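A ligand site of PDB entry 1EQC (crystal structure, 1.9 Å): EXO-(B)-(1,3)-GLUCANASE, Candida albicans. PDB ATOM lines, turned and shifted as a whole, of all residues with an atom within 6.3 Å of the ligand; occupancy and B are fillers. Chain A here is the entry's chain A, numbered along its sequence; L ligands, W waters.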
ATOM      1  N   GLU A  21     -16.483  20.001 -15.190  1.00  0.00           N
ATOM      2  CA  GLU A  21     -15.716  19.073 -14.352  1.00  0.00           C
ATOM      3  C   GLU A  21     -15.963  17.665 -14.865  1.00  0.00           C
ATOM      4  O   GLU A  21     -17.085  17.195 -14.826  1.00  0.00           O
ATOM      5  CB  GLU A  21     -16.152  19.207 -12.882  1.00  0.00           C
ATOM      6  CG  GLU A  21     -15.881  20.656 -12.396  1.00  0.00           C
ATOM      7  CD  GLU A  21     -15.849  20.741 -10.884  1.00  0.00           C
ATOM      8  OE1 GLU A  21     -15.368  19.763 -10.258  1.00  0.00           O
ATOM      9  OE2 GLU A  21     -16.330  21.780 -10.371  1.00  0.00           O
ATOM     10  N   TYR A  23     -15.679  14.643 -13.723  1.00  0.00           N
ATOM     11  CA  TYR A  23     -16.374  13.681 -12.907  1.00  0.00           C
ATOM     12  C   TYR A  23     -17.874  13.986 -12.730  1.00  0.00           C
ATOM     13  O   TYR A  23     -18.649  13.065 -12.444  1.00  0.00           O
ATOM     14  CB  TYR A  23     -15.719  13.481 -11.538  1.00  0.00           C
ATOM     15  CG  TYR A  23     -16.084  14.470 -10.443  1.00  0.00           C
ATOM     16  CD1 TYR A  23     -15.443  15.685 -10.330  1.00  0.00           C
ATOM     17  CD2 TYR A  23     -17.093  14.158  -9.535  1.00  0.00           C
ATOM     18  CE1 TYR A  23     -15.790  16.583  -9.309  1.00  0.00           C
ATOM     19  CE2 TYR A  23     -17.425  15.044  -8.510  1.00  0.00           C
ATOM     20  CZ  TYR A  23     -16.768  16.242  -8.415  1.00  0.00           C
ATOM     21  OH  TYR A  23     -17.127  17.125  -7.391  1.00  0.00           O
ATOM     22  N   MET A  24     -18.273  15.224 -12.956  1.00  0.00           N
ATOM     23  CA  MET A  24     -19.658  15.643 -12.777  1.00  0.00           C
ATOM     24  C   MET A  24     -20.463  15.462 -14.047  1.00  0.00           C
ATOM     25  O   MET A  24     -21.643  15.135 -13.986  1.00  0.00           O
ATOM     26  CB  MET A  24     -19.682  17.126 -12.357  1.00  0.00           C
ATOM     27  CG  MET A  24     -19.014  17.257 -10.969  1.00  0.00           C
ATOM     28  SD  MET A  24     -19.171  18.968 -10.381  1.00  0.00           S
ATOM     29  CE  MET A  24     -20.880  18.959  -9.835  1.00  0.00           C
ATOM     30  N   ARG A  86     -24.533  28.408  -4.059  1.00  0.00           N
ATOM     31  CA  ARG A  86     -23.192  28.972  -4.334  1.00  0.00           C
ATOM     32  C   ARG A  86     -22.951  28.734  -5.820  1.00  0.00           C
ATOM     33  O   ARG A  86     -23.157  27.601  -6.283  1.00  0.00           O
ATOM     34  CB  ARG A  86     -22.152  28.211  -3.500  1.00  0.00           C
ATOM     35  CG  ARG A  86     -20.704  28.637  -3.767  1.00  0.00           C
ATOM     36  CD  ARG A  86     -19.838  27.957  -2.677  1.00  0.00           C
ATOM     37  NE  ARG A  86     -18.437  28.286  -2.743  1.00  0.00           N
ATOM     38  CZ  ARG A  86     -17.495  27.449  -3.221  1.00  0.00           C
ATOM     39  NH1 ARG A  86     -17.858  26.250  -3.675  1.00  0.00           N
ATOM     40  NH2 ARG A  86     -16.238  27.856  -3.214  1.00  0.00           N
ATOM     41  N   PRO A  88     -20.303  28.690  -8.867  1.00  0.00           N
ATOM     42  CA  PRO A  88     -18.968  28.801  -9.382  1.00  0.00           C
ATOM     43  C   PRO A  88     -18.955  29.332 -10.806  1.00  0.00           C
ATOM     44  O   PRO A  88     -19.791  28.898 -11.642  1.00  0.00           O
ATOM     45  CB  PRO A  88     -18.451  27.341  -9.437  1.00  0.00           C
ATOM     46  CG  PRO A  88     -19.375  26.581  -8.534  1.00  0.00           C
ATOM     47  CD  PRO A  88     -20.712  27.294  -8.623  1.00  0.00           C
ATOM     48  N   ASP A 127     -18.960  32.848  -6.882  1.00  0.00           N
ATOM     49  CA  ASP A 127     -17.613  32.357  -6.509  1.00  0.00           C
ATOM     50  C   ASP A 127     -16.715  32.342  -7.734  1.00  0.00           C
ATOM     51  O   ASP A 127     -17.039  31.652  -8.691  1.00  0.00           O
ATOM     52  CB  ASP A 127     -17.815  30.937  -5.949  1.00  0.00           C
ATOM     53  CG  ASP A 127     -16.693  29.940  -6.198  1.00  0.00           C
ATOM     54  OD1 ASP A 127     -15.518  30.307  -6.124  1.00  0.00           O
ATOM     55  OD2 ASP A 127     -16.994  28.746  -6.468  1.00  0.00           O
ATOM     56  N   HIS A 129     -14.149  30.777  -9.456  1.00  0.00           N
ATOM     57  CA  HIS A 129     -13.673  29.413  -9.215  1.00  0.00           C
ATOM     58  C   HIS A 129     -12.367  29.098  -9.934  1.00  0.00           C
ATOM     59  O   HIS A 129     -11.700  28.131  -9.580  1.00  0.00           O
ATOM     60  CB  HIS A 129     -14.751  28.443  -9.690  1.00  0.00           C
ATOM     61  CG  HIS A 129     -14.899  27.173  -8.903  1.00  0.00           C
ATOM     62  ND1 HIS A 129     -15.391  27.111  -7.632  1.00  0.00           N
ATOM     63  CD2 HIS A 129     -14.606  25.893  -9.284  1.00  0.00           C
ATOM     64  CE1 HIS A 129     -15.431  25.846  -7.220  1.00  0.00           C
ATOM     65  NE2 HIS A 129     -14.936  25.089  -8.234  1.00  0.00           N
ATOM     66  N   PHE A 138      -5.995  22.240 -10.091  1.00  0.00           N
ATOM     67  CA  PHE A 138      -7.067  21.250 -10.186  1.00  0.00           C
ATOM     68  C   PHE A 138      -7.791  21.434 -11.524  1.00  0.00           C
ATOM     69  O   PHE A 138      -7.847  22.552 -12.043  1.00  0.00           O
ATOM     70  CB  PHE A 138      -8.093  21.407  -9.052  1.00  0.00           C
ATOM     71  CG  PHE A 138      -7.573  21.388  -7.640  1.00  0.00           C
ATOM     72  CD1 PHE A 138      -6.457  20.669  -7.270  1.00  0.00           C
ATOM     73  CD2 PHE A 138      -8.253  22.086  -6.640  1.00  0.00           C
ATOM     74  CE1 PHE A 138      -6.017  20.672  -5.965  1.00  0.00           C
ATOM     75  CE2 PHE A 138      -7.827  22.087  -5.336  1.00  0.00           C
ATOM     76  CZ  PHE A 138      -6.690  21.374  -4.986  1.00  0.00           C
ATOM     77  N   ASN A 140     -10.868  21.618 -11.905  1.00  0.00           N
ATOM     78  CA  ASN A 140     -11.990  22.559 -11.686  1.00  0.00           C
ATOM     79  C   ASN A 140     -11.597  24.014 -11.647  1.00  0.00           C
ATOM     80  O   ASN A 140     -12.471  24.904 -11.533  1.00  0.00           O
ATOM     81  CB  ASN A 140     -12.741  22.079 -10.444  1.00  0.00           C
ATOM     82  CG  ASN A 140     -11.809  22.013  -9.246  1.00  0.00           C
ATOM     83  OD1 ASN A 140     -11.348  23.033  -8.766  1.00  0.00           O
ATOM     84  ND2 ASN A 140     -11.578  20.800  -8.755  1.00  0.00           N
ATOM     85  N   SER A 141     -10.314  24.386 -11.724  1.00  0.00           N
ATOM     86  CA  SER A 141      -9.880  25.751 -11.880  1.00  0.00           C
ATOM     87  C   SER A 141      -9.899  26.126 -13.377  1.00  0.00           C
ATOM     88  O   SER A 141      -9.706  27.295 -13.696  1.00  0.00           O
ATOM     89  CB  SER A 141      -8.448  26.028 -11.405  1.00  0.00           C
ATOM     90  OG  SER A 141      -7.498  25.330 -12.256  1.00  0.00           O
ATOM     91  N   ASN A 185     -11.824  30.574  -5.333  1.00  0.00           N
ATOM     92  CA  ASN A 185     -12.043  29.246  -4.771  1.00  0.00           C
ATOM     93  C   ASN A 185     -10.736  28.481  -4.520  1.00  0.00           C
ATOM     94  O   ASN A 185      -9.889  28.458  -5.419  1.00  0.00           O
ATOM     95  CB  ASN A 185     -12.833  28.401  -5.813  1.00  0.00           C
ATOM     96  CG  ASN A 185     -13.081  27.007  -5.239  1.00  0.00           C
ATOM     97  OD1 ASN A 185     -13.736  26.897  -4.197  1.00  0.00           O
ATOM     98  ND2 ASN A 185     -12.554  26.006  -5.921  1.00  0.00           N
ATOM     99  N   GLU A 186     -10.553  27.918  -3.339  1.00  0.00           N
ATOM    100  CA  GLU A 186      -9.446  27.025  -3.038  1.00  0.00           C
ATOM    101  C   GLU A 186      -8.077  27.354  -3.573  1.00  0.00           C
ATOM    102  O   GLU A 186      -7.451  26.551  -4.300  1.00  0.00           O
ATOM    103  CB  GLU A 186      -9.839  25.584  -3.528  1.00  0.00           C
ATOM    104  CG  GLU A 186     -11.039  25.012  -2.769  1.00  0.00           C
ATOM    105  CD  GLU A 186     -11.209  23.530  -2.808  1.00  0.00           C
ATOM    106  OE1 GLU A 186     -10.422  22.812  -3.486  1.00  0.00           O
ATOM    107  OE2 GLU A 186     -12.120  22.981  -2.137  1.00  0.00           O
ATOM    108  N   HIS A 247     -13.809  24.334   3.436  1.00  0.00           N
ATOM    109  CA  HIS A 247     -14.324  23.172   2.696  1.00  0.00           C
ATOM    110  C   HIS A 247     -13.906  21.921   3.484  1.00  0.00           C
ATOM    111  O   HIS A 247     -12.790  21.903   3.996  1.00  0.00           O
ATOM    112  CB  HIS A 247     -13.717  23.090   1.292  1.00  0.00           C
ATOM    113  CG  HIS A 247     -14.216  24.240   0.439  1.00  0.00           C
ATOM    114  ND1 HIS A 247     -13.799  24.464  -0.855  1.00  0.00           N
ATOM    115  CD2 HIS A 247     -15.100  25.205   0.721  1.00  0.00           C
ATOM    116  CE1 HIS A 247     -14.437  25.557  -1.324  1.00  0.00           C
ATOM    117  NE2 HIS A 247     -15.233  26.015  -0.373  1.00  0.00           N
ATOM    118  N   TYR A 249     -13.673  17.674   3.676  1.00  0.00           N
ATOM    119  CA  TYR A 249     -13.876  16.328   3.121  1.00  0.00           C
ATOM    120  C   TYR A 249     -12.958  15.317   3.817  1.00  0.00           C
ATOM    121  O   TYR A 249     -11.988  15.717   4.479  1.00  0.00           O
ATOM    122  CB  TYR A 249     -13.499  16.333   1.654  1.00  0.00           C
ATOM    123  CG  TYR A 249     -14.370  17.180   0.757  1.00  0.00           C
ATOM    124  CD1 TYR A 249     -15.613  16.669   0.353  1.00  0.00           C
ATOM    125  CD2 TYR A 249     -13.980  18.436   0.366  1.00  0.00           C
ATOM    126  CE1 TYR A 249     -16.419  17.437  -0.466  1.00  0.00           C
ATOM    127  CE2 TYR A 249     -14.801  19.216  -0.456  1.00  0.00           C
ATOM    128  CZ  TYR A 249     -16.007  18.687  -0.866  1.00  0.00           C
ATOM    129  OH  TYR A 249     -16.807  19.404  -1.726  1.00  0.00           O
ATOM    130  N   PHE A 252      -9.458  12.540   0.426  1.00  0.00           N
ATOM    131  CA  PHE A 252      -8.361  12.830  -0.496  1.00  0.00           C
ATOM    132  C   PHE A 252      -6.998  12.381  -0.029  1.00  0.00           C
ATOM    133  O   PHE A 252      -5.991  12.948  -0.435  1.00  0.00           O
ATOM    134  CB  PHE A 252      -8.358  14.304  -0.929  1.00  0.00           C
ATOM    135  CG  PHE A 252      -9.552  14.597  -1.811  1.00  0.00           C
ATOM    136  CD1 PHE A 252      -9.694  14.012  -3.037  1.00  0.00           C
ATOM    137  CD2 PHE A 252     -10.540  15.467  -1.361  1.00  0.00           C
ATOM    138  CE1 PHE A 252     -10.799  14.272  -3.839  1.00  0.00           C
ATOM    139  CE2 PHE A 252     -11.646  15.729  -2.153  1.00  0.00           C
ATOM    140  CZ  PHE A 252     -11.786  15.126  -3.396  1.00  0.00           C
ATOM    141  N   GLU A 286     -18.342  23.882   1.109  1.00  0.00           N
ATOM    142  CA  GLU A 286     -18.320  22.627   0.412  1.00  0.00           C
ATOM    143  C   GLU A 286     -18.134  21.471   1.410  1.00  0.00           C
ATOM    144  O   GLU A 286     -17.379  21.600   2.363  1.00  0.00           O
ATOM    145  CB  GLU A 286     -17.181  22.476  -0.609  1.00  0.00           C
ATOM    146  CG  GLU A 286     -17.262  23.339  -1.834  1.00  0.00           C
ATOM    147  CD  GLU A 286     -16.247  22.967  -2.907  1.00  0.00           C
ATOM    148  OE1 GLU A 286     -15.797  21.791  -2.916  1.00  0.00           O
ATOM    149  OE2 GLU A 286     -15.917  23.822  -3.732  1.00  0.00           O
ATOM    150  N   LEU A 298     -12.891  11.581 -10.338  1.00  0.00           N
ATOM    151  CA  LEU A 298     -12.879  12.573  -9.254  1.00  0.00           C
ATOM    152  C   LEU A 298     -11.487  13.164  -9.044  1.00  0.00           C
ATOM    153  O   LEU A 298     -11.286  14.359  -8.786  1.00  0.00           O
ATOM    154  CB  LEU A 298     -13.325  11.905  -7.958  1.00  0.00           C
ATOM    155  CG  LEU A 298     -13.333  12.751  -6.683  1.00  0.00           C
ATOM    156  CD1 LEU A 298     -14.346  13.883  -6.813  1.00  0.00           C
ATOM    157  CD2 LEU A 298     -13.638  11.847  -5.491  1.00  0.00           C
ATOM    158  N   TRP A 357     -21.735  20.039  -1.835  1.00  0.00           N
ATOM    159  CA  TRP A 357     -21.217  19.929  -3.226  1.00  0.00           C
ATOM    160  C   TRP A 357     -21.611  18.564  -3.731  1.00  0.00           C
ATOM    161  O   TRP A 357     -21.108  17.530  -3.256  1.00  0.00           O
ATOM    162  CB  TRP A 357     -19.652  20.058  -3.219  1.00  0.00           C
ATOM    163  CG  TRP A 357     -19.218  20.070  -4.676  1.00  0.00           C
ATOM    164  CD1 TRP A 357     -19.100  18.981  -5.474  1.00  0.00           C
ATOM    165  CD2 TRP A 357     -18.948  21.211  -5.486  1.00  0.00           C
ATOM    166  NE1 TRP A 357     -18.739  19.380  -6.762  1.00  0.00           N
ATOM    167  CE2 TRP A 357     -18.654  20.740  -6.784  1.00  0.00           C
ATOM    168  CE3 TRP A 357     -18.903  22.593  -5.259  1.00  0.00           C
ATOM    169  CZ2 TRP A 357     -18.315  21.587  -7.842  1.00  0.00           C
ATOM    170  CZ3 TRP A 357     -18.569  23.422  -6.293  1.00  0.00           C
ATOM    171  CH2 TRP A 357     -18.280  22.929  -7.587  1.00  0.00           C
ATOM    172  N   TRP A 367     -21.986  12.596  -4.573  1.00  0.00           N
ATOM    173  CA  TRP A 367     -21.792  14.007  -4.836  1.00  0.00           C
ATOM    174  C   TRP A 367     -23.067  14.700  -5.368  1.00  0.00           C
ATOM    175  O   TRP A 367     -22.989  15.823  -5.895  1.00  0.00           O
ATOM    176  CB  TRP A 367     -20.679  14.102  -5.913  1.00  0.00           C
ATOM    177  CG  TRP A 367     -19.371  13.510  -5.410  1.00  0.00           C
ATOM    178  CD1 TRP A 367     -18.910  12.242  -5.595  1.00  0.00           C
ATOM    179  CD2 TRP A 367     -18.405  14.183  -4.606  1.00  0.00           C
ATOM    180  NE1 TRP A 367     -17.693  12.073  -4.949  1.00  0.00           N
ATOM    181  CE2 TRP A 367     -17.365  13.263  -4.332  1.00  0.00           C
ATOM    182  CE3 TRP A 367     -18.302  15.477  -4.075  1.00  0.00           C
ATOM    183  CZ2 TRP A 367     -16.261  13.596  -3.571  1.00  0.00           C
ATOM    184  CZ3 TRP A 367     -17.197  15.808  -3.324  1.00  0.00           C
ATOM    185  CH2 TRP A 367     -16.178  14.875  -3.069  1.00  0.00           C
HETATM  186  C1  LIG L   1     -13.133  21.287  -5.050  1.00  0.00           C
HETATM  187  C2  LIG L   1     -13.693  22.289  -6.070  1.00  0.00           C
HETATM  188  C3  LIG L   1     -14.904  21.695  -6.814  1.00  0.00           C
HETATM  189  C4  LIG L   1     -14.715  20.187  -6.889  1.00  0.00           C
HETATM  190  C5  LIG L   1     -14.842  19.591  -5.476  1.00  0.00           C
HETATM  191  C6  LIG L   1     -14.383  18.129  -5.278  1.00  0.00           C
HETATM  192  O1  LIG L   1     -14.058  23.500  -5.444  1.00  0.00           O
HETATM  193  O2  LIG L   1     -14.886  22.250  -8.151  1.00  0.00           O
HETATM  194  O3  LIG L   1     -15.687  19.555  -7.702  1.00  0.00           O
HETATM  195  O4  LIG L   1     -13.080  17.948  -5.830  1.00  0.00           O
HETATM  196  N1  LIG L   1     -14.154  20.390  -4.500  1.00  0.00           N
HETATM  197  C7  LIG L   1     -14.306  18.118  -3.726  1.00  0.00           C
HETATM  198  C8  LIG L   1     -13.546  19.473  -3.515  1.00  0.00           C
HETATM  199  O   HOH W   1     -12.525  16.716  -8.066  1.00  0.00           O
HETATM  200  O   HOH W   2     -10.290  19.259  -6.402  1.00  0.00           O
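The side-chain carboxylate of Glu 286 is in salt-bridge range of a nitrogen (N1) of the ligand. An oxygen (O3) of the ligand is in hydrogen-bond range of the side-chain carboxylate (OE1) of Glu 21, 2.6 Å away. A ring nitrogen (NE2) of His 129 lies within hydrogen-bond range of an oxygen (O2) of the ligand (2.8 Å). OH of Tyr 23 lies within hydrogen-bond range of O3 of the ligand. An oxygen (O1) of the ligand is in hydrogen-bond range of the side-chain amide nitrogen of Asn 185. The indole nitrogen of Trp 357 is in hydrogen-bond range of an oxygen (O3) of the ligand, 3.2 Å away.
OE1 of Glu 286 is in hydrogen-bond range of OH of Tyr 249. The guanidinium group (NH1) of Arg 86 lies within salt-bridge range of the side-chain carboxylate (OE2) of Glu 286. ND2 of Asn 185 sits close to NE2 of His 129 (3.4 Å). ND1 of His 129 is in hydrogen-bond range of OD2 of Asp 127 (2.6 Å). NE1 of Trp 357 is in hydrogen-bond range of OH of Tyr 23, at 2.8 Å. NH2 of Arg 86 lies within hydrogen-bond range of OD1 of Asn 185, 2.9 Å away. NE1 of Trp 357 sits at hydrogen-bond distance from SD of Met 24. ND1 of His 247 is in hydrogen-bond range of OE2 of Glu 186 (2.6 Å).
CB of Asn 140 touches O2 of the ligand (3.1 Å). Glu 186 touches the ligand. Tyr 249 touches the ligand (CE2 to C8, 3.3 Å). Phe 252 touches the ligand. CZ3 of Trp 367 touches C7 of the ligand, 3.7 Å away. Hydrophobic or aromatic side chains within 4 Å of the ligand: Tyr 23, His 129, Tyr 249, Phe 252, Trp 357 and Trp 367.
Water W1 lies within hydrogen-bond range of an oxygen (O4) of the ligand (2.6 Å) and the backbone carbonyl oxygen (O) of Leu 298 (2.8 Å). Water W2 bridges ND2 of Asn 140 (3.1 Å) and O4 of the ligand (3.1 Å).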
